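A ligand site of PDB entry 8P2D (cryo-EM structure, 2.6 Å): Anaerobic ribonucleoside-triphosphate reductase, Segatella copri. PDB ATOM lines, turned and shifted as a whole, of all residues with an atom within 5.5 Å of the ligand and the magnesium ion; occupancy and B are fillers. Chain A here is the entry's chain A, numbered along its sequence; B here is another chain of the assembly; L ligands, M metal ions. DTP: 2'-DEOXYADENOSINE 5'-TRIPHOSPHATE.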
ATOM      1  N   PHE A 188     -13.601 -31.286  27.062  1.00  0.00           N
ATOM      2  CA  PHE A 188     -12.503 -31.147  26.125  1.00  0.00           C
ATOM      3  C   PHE A 188     -11.915 -29.744  26.249  1.00  0.00           C
ATOM      4  O   PHE A 188     -12.643 -28.770  26.489  1.00  0.00           O
ATOM      5  CB  PHE A 188     -12.940 -31.415  24.677  1.00  0.00           C
ATOM      6  CG  PHE A 188     -13.665 -30.266  24.032  1.00  0.00           C
ATOM      7  CD1 PHE A 188     -15.025 -30.069  24.266  1.00  0.00           C
ATOM      8  CD2 PHE A 188     -13.012 -29.404  23.175  1.00  0.00           C
ATOM      9  CE1 PHE A 188     -15.692 -29.021  23.673  1.00  0.00           C
ATOM     10  CE2 PHE A 188     -13.686 -28.354  22.575  1.00  0.00           C
ATOM     11  CZ  PHE A 188     -15.026 -28.164  22.830  1.00  0.00           C
ATOM     12  N   SER A 194     -12.340 -24.442  26.992  1.00  0.00           N
ATOM     13  CA  SER A 194     -12.479 -25.342  28.138  1.00  0.00           C
ATOM     14  C   SER A 194     -13.964 -25.620  28.361  1.00  0.00           C
ATOM     15  O   SER A 194     -14.744 -24.709  28.654  1.00  0.00           O
ATOM     16  CB  SER A 194     -11.846 -24.723  29.379  1.00  0.00           C
ATOM     17  OG  SER A 194     -11.917 -25.598  30.486  1.00  0.00           O
ATOM     18  N   SER A 195     -14.353 -26.889  28.216  1.00  0.00           N
ATOM     19  CA  SER A 195     -15.750 -27.299  28.287  1.00  0.00           C
ATOM     20  C   SER A 195     -15.966 -28.242  29.459  1.00  0.00           C
ATOM     21  O   SER A 195     -15.187 -29.172  29.659  1.00  0.00           O
ATOM     22  CB  SER A 195     -16.185 -27.972  26.988  1.00  0.00           C
ATOM     23  OG  SER A 195     -17.501 -28.481  27.092  1.00  0.00           O
ATOM     24  N   ARG A 196     -17.023 -27.997  30.229  1.00  0.00           N
ATOM     25  CA  ARG A 196     -17.440 -28.874  31.299  1.00  0.00           C
ATOM     26  C   ARG A 196     -18.224 -30.058  30.732  1.00  0.00           C
ATOM     27  O   ARG A 196     -18.712 -30.013  29.604  1.00  0.00           O
ATOM     28  CB  ARG A 196     -18.274 -28.101  32.314  1.00  0.00           C
ATOM     29  CG  ARG A 196     -17.494 -27.045  33.088  1.00  0.00           C
ATOM     30  CD  ARG A 196     -18.396 -26.237  33.997  1.00  0.00           C
ATOM     31  NE  ARG A 196     -19.340 -25.413  33.241  1.00  0.00           N
ATOM     32  CZ  ARG A 196     -19.080 -24.180  32.824  1.00  0.00           C
ATOM     33  NH1 ARG A 196     -17.924 -23.592  33.059  1.00  0.00           N
ATOM     34  NH2 ARG A 196     -20.008 -23.521  32.137  1.00  0.00           N
ATOM     35  N   PRO A 197     -18.354 -31.141  31.515  1.00  0.00           N
ATOM     36  CA  PRO A 197     -19.125 -32.297  31.031  1.00  0.00           C
ATOM     37  C   PRO A 197     -20.586 -31.966  30.763  1.00  0.00           C
ATOM     38  O   PRO A 197     -21.174 -31.081  31.403  1.00  0.00           O
ATOM     39  CB  PRO A 197     -18.984 -33.314  32.176  1.00  0.00           C
ATOM     40  CG  PRO A 197     -17.724 -32.928  32.857  1.00  0.00           C
ATOM     41  CD  PRO A 197     -17.635 -31.445  32.763  1.00  0.00           C
ATOM     42  N   ALA A 198     -21.166 -32.676  29.803  1.00  0.00           N
ATOM     43  CA  ALA A 198     -22.545 -32.460  29.395  1.00  0.00           C
ATOM     44  C   ALA A 198     -23.517 -32.893  30.492  1.00  0.00           C
ATOM     45  O   ALA A 198     -23.164 -33.611  31.425  1.00  0.00           O
ATOM     46  CB  ALA A 198     -22.854 -33.219  28.106  1.00  0.00           C
ATOM     47  N   LYS A 199     -24.767 -32.432  30.372  1.00  0.00           N
ATOM     48  CA  LYS A 199     -25.760 -32.672  31.415  1.00  0.00           C
ATOM     49  C   LYS A 199     -27.080 -33.218  30.885  1.00  0.00           C
ATOM     50  O   LYS A 199     -27.807 -33.886  31.625  1.00  0.00           O
ATOM     51  CB  LYS A 199     -26.004 -31.388  32.203  1.00  0.00           C
ATOM     52  CG  LYS A 199     -24.879 -30.999  33.145  1.00  0.00           C
ATOM     53  CD  LYS A 199     -24.804 -31.940  34.334  1.00  0.00           C
ATOM     54  CE  LYS A 199     -23.815 -31.440  35.368  1.00  0.00           C
ATOM     55  NZ  LYS A 199     -23.763 -32.320  36.571  1.00  0.00           N
ATOM     56  N   ARG A 200     -27.417 -32.944  29.631  1.00  0.00           N
ATOM     57  CA  ARG A 200     -28.731 -33.285  29.111  1.00  0.00           C
ATOM     58  C   ARG A 200     -28.640 -33.565  27.615  1.00  0.00           C
ATOM     59  O   ARG A 200     -27.567 -33.419  27.008  1.00  0.00           O
ATOM     60  CB  ARG A 200     -29.741 -32.171  29.417  1.00  0.00           C
ATOM     61  CG  ARG A 200     -29.260 -30.791  29.005  1.00  0.00           C
ATOM     62  CD  ARG A 200     -30.092 -29.701  29.656  1.00  0.00           C
ATOM     63  NE  ARG A 200     -29.474 -28.390  29.458  1.00  0.00           N
ATOM     64  CZ  ARG A 200     -28.506 -27.897  30.216  1.00  0.00           C
ATOM     65  NH1 ARG A 200     -28.026 -28.579  31.243  1.00  0.00           N
ATOM     66  NH2 ARG A 200     -28.009 -26.699  29.934  1.00  0.00           N
ATOM     67  N   THR A 203     -27.490 -30.575  25.342  1.00  0.00           N
ATOM     68  CA  THR A 203     -26.065 -30.337  25.477  1.00  0.00           C
ATOM     69  C   THR A 203     -25.245 -31.494  24.924  1.00  0.00           C
ATOM     70  O   THR A 203     -24.239 -31.278  24.235  1.00  0.00           O
ATOM     71  CB  THR A 203     -25.708 -30.076  26.939  1.00  0.00           C
ATOM     72  OG1 THR A 203     -26.363 -28.896  27.394  1.00  0.00           O
ATOM     73  CG2 THR A 203     -24.205 -29.911  27.091  1.00  0.00           C
ATOM     74  N   VAL A 206     -25.461 -31.468  21.048  1.00  0.00           N
ATOM     75  CA  VAL A 206     -24.687 -30.357  20.502  1.00  0.00           C
ATOM     76  C   VAL A 206     -23.198 -30.597  20.693  1.00  0.00           C
ATOM     77  O   VAL A 206     -22.395 -30.235  19.834  1.00  0.00           O
ATOM     78  CB  VAL A 206     -25.144 -29.021  21.124  1.00  0.00           C
ATOM     79  CG1 VAL A 206     -24.238 -27.889  20.689  1.00  0.00           C
ATOM     80  CG2 VAL A 206     -26.580 -28.730  20.723  1.00  0.00           C
ATOM     81  N   LEU A 207     -22.796 -31.223  21.808  1.00  0.00           N
ATOM     82  CA  LEU A 207     -21.395 -31.560  22.003  1.00  0.00           C
ATOM     83  C   LEU A 207     -20.934 -32.624  21.027  1.00  0.00           C
ATOM     84  O   LEU A 207     -19.796 -32.597  20.570  1.00  0.00           O
ATOM     85  CB  LEU A 207     -21.159 -32.022  23.448  1.00  0.00           C
ATOM     86  CG  LEU A 207     -20.781 -30.946  24.466  1.00  0.00           C
ATOM     87  CD1 LEU A 207     -20.450 -31.585  25.806  1.00  0.00           C
ATOM     88  CD2 LEU A 207     -19.617 -30.118  23.958  1.00  0.00           C
ATOM     89  N   ILE A 210     -20.382 -30.763  17.887  1.00  0.00           N
ATOM     90  CA  ILE A 210     -19.163 -29.967  17.984  1.00  0.00           C
ATOM     91  C   ILE A 210     -17.934 -30.850  17.867  1.00  0.00           C
ATOM     92  O   ILE A 210     -16.945 -30.485  17.244  1.00  0.00           O
ATOM     93  CB  ILE A 210     -19.169 -29.157  19.296  1.00  0.00           C
ATOM     94  CG1 ILE A 210     -20.215 -28.043  19.232  1.00  0.00           C
ATOM     95  CG2 ILE A 210     -17.795 -28.568  19.571  1.00  0.00           C
ATOM     96  CD1 ILE A 210     -19.998 -27.054  18.116  1.00  0.00           C
ATOM     97  N   HIS B 293     -31.162 -18.374  29.606  1.00  0.00           N
ATOM     98  CA  HIS B 293     -29.821 -18.308  30.174  1.00  0.00           C
ATOM     99  C   HIS B 293     -28.934 -19.430  29.628  1.00  0.00           C
ATOM    100  O   HIS B 293     -27.775 -19.199  29.293  1.00  0.00           O
ATOM    101  CB  HIS B 293     -29.905 -18.369  31.698  1.00  0.00           C
ATOM    102  CG  HIS B 293     -28.718 -19.029  32.348  1.00  0.00           C
ATOM    103  ND1 HIS B 293     -27.426 -18.588  32.159  1.00  0.00           N
ATOM    104  CD2 HIS B 293     -28.643 -20.084  33.191  1.00  0.00           C
ATOM    105  CE1 HIS B 293     -26.608 -19.354  32.853  1.00  0.00           C
ATOM    106  NE2 HIS B 293     -27.318 -20.267  33.494  1.00  0.00           N
ATOM    107  N   GLN B 294     -29.463 -20.651  29.543  1.00  0.00           N
ATOM    108  CA  GLN B 294     -28.712 -21.736  28.937  1.00  0.00           C
ATOM    109  C   GLN B 294     -28.445 -21.454  27.464  1.00  0.00           C
ATOM    110  O   GLN B 294     -27.367 -21.772  26.955  1.00  0.00           O
ATOM    111  CB  GLN B 294     -29.450 -23.058  29.101  1.00  0.00           C
ATOM    112  CG  GLN B 294     -29.722 -23.477  30.546  1.00  0.00           C
ATOM    113  CD  GLN B 294     -28.475 -23.899  31.293  1.00  0.00           C
ATOM    114  OE1 GLN B 294     -27.394 -24.020  30.711  1.00  0.00           O
ATOM    115  NE2 GLN B 294     -28.606 -24.134  32.591  1.00  0.00           N
ATOM    116  N   GLU B 297     -25.630 -18.948  27.385  1.00  0.00           N
ATOM    117  CA  GLU B 297     -24.385 -19.608  27.747  1.00  0.00           C
ATOM    118  C   GLU B 297     -23.848 -20.442  26.588  1.00  0.00           C
ATOM    119  O   GLU B 297     -22.644 -20.448  26.311  1.00  0.00           O
ATOM    120  CB  GLU B 297     -24.582 -20.466  28.986  1.00  0.00           C
ATOM    121  CG  GLU B 297     -23.410 -21.380  29.311  1.00  0.00           C
ATOM    122  CD  GLU B 297     -23.607 -22.147  30.597  1.00  0.00           C
ATOM    123  OE1 GLU B 297     -24.385 -21.689  31.453  1.00  0.00           O
ATOM    124  OE2 GLU B 297     -22.975 -23.210  30.758  1.00  0.00           O
ATOM    125  N   ALA B 298     -24.736 -21.168  25.899  1.00  0.00           N
ATOM    126  CA  ALA B 298     -24.330 -21.901  24.713  1.00  0.00           C
ATOM    127  C   ALA B 298     -23.847 -20.951  23.623  1.00  0.00           C
ATOM    128  O   ALA B 298     -22.876 -21.241  22.930  1.00  0.00           O
ATOM    129  CB  ALA B 298     -25.482 -22.757  24.203  1.00  0.00           C
ATOM    130  N   PHE B 299     -24.508 -19.800  23.491  1.00  0.00           N
ATOM    131  CA  PHE B 299     -24.069 -18.788  22.531  1.00  0.00           C
ATOM    132  C   PHE B 299     -22.658 -18.306  22.847  1.00  0.00           C
ATOM    133  O   PHE B 299     -21.837 -18.143  21.945  1.00  0.00           O
ATOM    134  CB  PHE B 299     -25.063 -17.615  22.538  1.00  0.00           C
ATOM    135  CG  PHE B 299     -24.644 -16.455  21.689  1.00  0.00           C
ATOM    136  CD1 PHE B 299     -24.942 -16.417  20.333  1.00  0.00           C
ATOM    137  CD2 PHE B 299     -23.963 -15.373  22.242  1.00  0.00           C
ATOM    138  CE1 PHE B 299     -24.565 -15.346  19.560  1.00  0.00           C
ATOM    139  CE2 PHE B 299     -23.586 -14.312  21.467  1.00  0.00           C
ATOM    140  CZ  PHE B 299     -23.886 -14.287  20.121  1.00  0.00           C
ATOM    141  N   HIS B 301     -20.329 -20.017  24.605  1.00  0.00           N
ATOM    142  CA  HIS B 301     -19.421 -21.132  24.334  1.00  0.00           C
ATOM    143  C   HIS B 301     -19.316 -21.413  22.839  1.00  0.00           C
ATOM    144  O   HIS B 301     -18.207 -21.641  22.334  1.00  0.00           O
ATOM    145  CB  HIS B 301     -19.885 -22.382  25.068  1.00  0.00           C
ATOM    146  CG  HIS B 301     -19.609 -22.358  26.549  1.00  0.00           C
ATOM    147  ND1 HIS B 301     -18.364 -22.635  27.069  1.00  0.00           N
ATOM    148  CD2 HIS B 301     -20.418 -22.096  27.600  1.00  0.00           C
ATOM    149  CE1 HIS B 301     -18.420 -22.530  28.391  1.00  0.00           C
ATOM    150  NE2 HIS B 301     -19.652 -22.207  28.734  1.00  0.00           N
ATOM    151  N   ASN B 302     -20.433 -21.393  22.114  1.00  0.00           N
ATOM    152  CA  ASN B 302     -20.392 -21.700  20.695  1.00  0.00           C
ATOM    153  C   ASN B 302     -19.558 -20.688  19.922  1.00  0.00           C
ATOM    154  O   ASN B 302     -18.858 -21.053  18.974  1.00  0.00           O
ATOM    155  CB  ASN B 302     -21.810 -21.756  20.117  1.00  0.00           C
ATOM    156  CG  ASN B 302     -21.849 -22.354  18.724  1.00  0.00           C
ATOM    157  OD1 ASN B 302     -21.612 -21.671  17.735  1.00  0.00           O
ATOM    158  ND2 ASN B 302     -22.137 -23.649  18.646  1.00  0.00           N
ATOM    159  N   THR B 305     -15.787 -21.704  21.196  1.00  0.00           N
ATOM    160  CA  THR B 305     -15.168 -22.979  20.838  1.00  0.00           C
ATOM    161  C   THR B 305     -14.580 -22.858  19.436  1.00  0.00           C
ATOM    162  O   THR B 305     -15.079 -23.415  18.457  1.00  0.00           O
ATOM    163  CB  THR B 305     -16.164 -24.124  20.961  1.00  0.00           C
ATOM    164  OG1 THR B 305     -15.598 -25.323  20.414  1.00  0.00           O
ATOM    165  CG2 THR B 305     -17.473 -23.806  20.233  1.00  0.00           C
ATOM    166  N   GLN B 342     -19.153 -15.540  34.988  1.00  0.00           N
ATOM    167  CA  GLN B 342     -18.859 -16.876  35.496  1.00  0.00           C
ATOM    168  C   GLN B 342     -17.640 -17.465  34.796  1.00  0.00           C
ATOM    169  O   GLN B 342     -16.775 -18.068  35.449  1.00  0.00           O
ATOM    170  CB  GLN B 342     -20.071 -17.788  35.326  1.00  0.00           C
ATOM    171  CG  GLN B 342     -21.336 -17.255  35.979  1.00  0.00           C
ATOM    172  CD  GLN B 342     -22.568 -18.053  35.587  1.00  0.00           C
ATOM    173  OE1 GLN B 342     -22.465 -19.066  34.882  1.00  0.00           O
ATOM    174  NE2 GLN B 342     -23.730 -17.608  36.034  1.00  0.00           N
ATOM    175  N   GLY B 345     -15.308 -23.084  31.206  1.00  0.00           N
ATOM    176  CA  GLY B 345     -14.515 -24.111  31.874  1.00  0.00           C
ATOM    177  C   GLY B 345     -14.634 -24.030  33.382  1.00  0.00           C
ATOM    178  O   GLY B 345     -15.705 -23.757  33.938  1.00  0.00           O
HETATM  179  PG  DTP L   1     -25.491 -26.310  33.983  1.00  0.00           P
HETATM  180  O1G DTP L   1     -26.873 -26.770  33.691  1.00  0.00           O
HETATM  181  O2G DTP L   1     -25.236 -26.060  35.478  1.00  0.00           O
HETATM  182  O3G DTP L   1     -25.074 -25.062  33.194  1.00  0.00           O
HETATM  183  PB  DTP L   1     -23.051 -27.529  32.843  1.00  0.00           P
HETATM  184  O1B DTP L   1     -22.424 -28.848  33.032  1.00  0.00           O
HETATM  185  O2B DTP L   1     -22.196 -26.340  33.292  1.00  0.00           O
HETATM  186  O3B DTP L   1     -24.432 -27.410  33.568  1.00  0.00           O
HETATM  187  PA  DTP L   1     -23.879 -28.113  30.069  1.00  0.00           P
HETATM  188  O1A DTP L   1     -23.963 -29.555  30.395  1.00  0.00           O
HETATM  189  O2A DTP L   1     -25.145 -27.496  29.490  1.00  0.00           O
HETATM  190  O3A DTP L   1     -23.473 -27.252  31.334  1.00  0.00           O
HETATM  191  O5' DTP L   1     -22.672 -27.819  29.101  1.00  0.00           O
HETATM  192  C5' DTP L   1     -21.544 -27.034  29.539  1.00  0.00           C
HETATM  193  C4' DTP L   1     -20.521 -27.023  28.445  1.00  0.00           C
HETATM  194  O4' DTP L   1     -21.132 -27.426  27.204  1.00  0.00           O
HETATM  195  C3' DTP L   1     -19.900 -25.669  28.163  1.00  0.00           C
HETATM  196  O3' DTP L   1     -18.767 -25.462  29.007  1.00  0.00           O
HETATM  197  C2' DTP L   1     -19.469 -25.800  26.704  1.00  0.00           C
HETATM  198  C1' DTP L   1     -20.448 -26.808  26.124  1.00  0.00           C
HETATM  199  N9  DTP L   1     -21.453 -26.251  25.220  1.00  0.00           N
HETATM  200  C8  DTP L   1     -22.764 -25.969  25.510  1.00  0.00           C
HETATM  201  N7  DTP L   1     -23.434 -25.471  24.493  1.00  0.00           N
HETATM  202  C5  DTP L   1     -22.504 -25.422  23.482  1.00  0.00           C
HETATM  203  C6  DTP L   1     -22.587 -25.000  22.134  1.00  0.00           C
HETATM  204  N6  DTP L   1     -23.696 -24.516  21.576  1.00  0.00           N
HETATM  205  N1  DTP L   1     -21.471 -25.078  21.383  1.00  0.00           N
HETATM  206  C2  DTP L   1     -20.354 -25.560  21.935  1.00  0.00           C
HETATM  207  N3  DTP L   1     -20.160 -25.995  23.178  1.00  0.00           N
HETATM  208  C4  DTP L   1     -21.273 -25.900  23.904  1.00  0.00           C
HETATM  209 MG    MG M   1     -23.777 -23.668  32.706  1.00  0.00          MG
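The backbone NH of Ser 195 lies within hydrogen-bond range of the backbone carbonyl oxygen of Phe 188, 3.1 Å away.
OE2 of Glu 297 of chain B sits close to NH2 of Arg 196 (3.3 Å).
The guanidinium group (NH2) of Arg 200 sits at hydrogen-bond distance from the side-chain amide oxygen (OE1) of Gln 294 of chain B (2.9 Å).
O3G of the ligand is bound to the magnesium ion, 2.0 Å away.
The magnesium ion is bound by OE2 of Glu 297 of chain B (2.2 Å).
The magnesium ion is bound by the side-chain carboxylate (OE1) of Glu 297 of chain B (2.4 Å).
The magnesium ion has three donor atoms within binding distance.
The backbone carbonyl oxygen (O) of Pro 197 sits close to an oxygen (O1B) of the ligand.
NE of Arg 196 lies within salt-bridge range of O2B of the ligand (3.0 Å).
A nitrogen (N1) of the ligand sits at hydrogen-bond distance from the side-chain amide nitrogen (ND2) of Asn 302 of chain B (3.2 Å).
An oxygen (O1G) of the ligand sits at hydrogen-bond distance from the side-chain amide nitrogen (NE2) of Gln 294 of chain B.
The guanidinium group (NH2) of Arg 200 is in salt-bridge range of an oxygen (O2A) of the ligand (3.0 Å).
The side-chain hydroxyl (OG1) of Thr 203 lies within hydrogen-bond range of an oxygen (O2A) of the ligand (2.8 Å).
N of Arg 196 sits at hydrogen-bond distance from O3' of the ligand (3.3 Å).
The backbone NH (N) of Lys 199 is in hydrogen-bond range of an oxygen (O1A) of the ligand (3.0 Å).
O3' of the ligand lies close to NE2 of His 301 of chain B (3.4 Å).
Ser 195 touches the ligand.
Ala 198 touches the ligand (C to O1A, 3.4 Å).
Val 206 touches the ligand (CG1 to N6, 3.5 Å).
CG1 of Ile 210 touches C2 of the ligand (3.7 Å).
Ala 298 of chain B touches the ligand (CB to N7, 3.4 Å).
Thr 305 of chain B touches the ligand (CG2 to C2, 3.8 Å).
Hydrophobic or aromatic side chains within 4 Å of the ligand: Val 206, Ile 210, Ala 298 of chain B and His 301 of chain B.
15 residues have an atom within 4 Å of the ligand: Ser 195, Arg 196, Pro 197, Ala 198, Lys 199, Arg 200, Thr 203, Val 206, Ile 210, Gln 294 of chain B, Glu 297 of chain B, Ala 298 of chain B, His 301 of chain B, Asn 302 of chain B and Thr 305 of chain B.
Arg 196 touches the magnesium ion (NH2 to MG, 3.8 Å).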
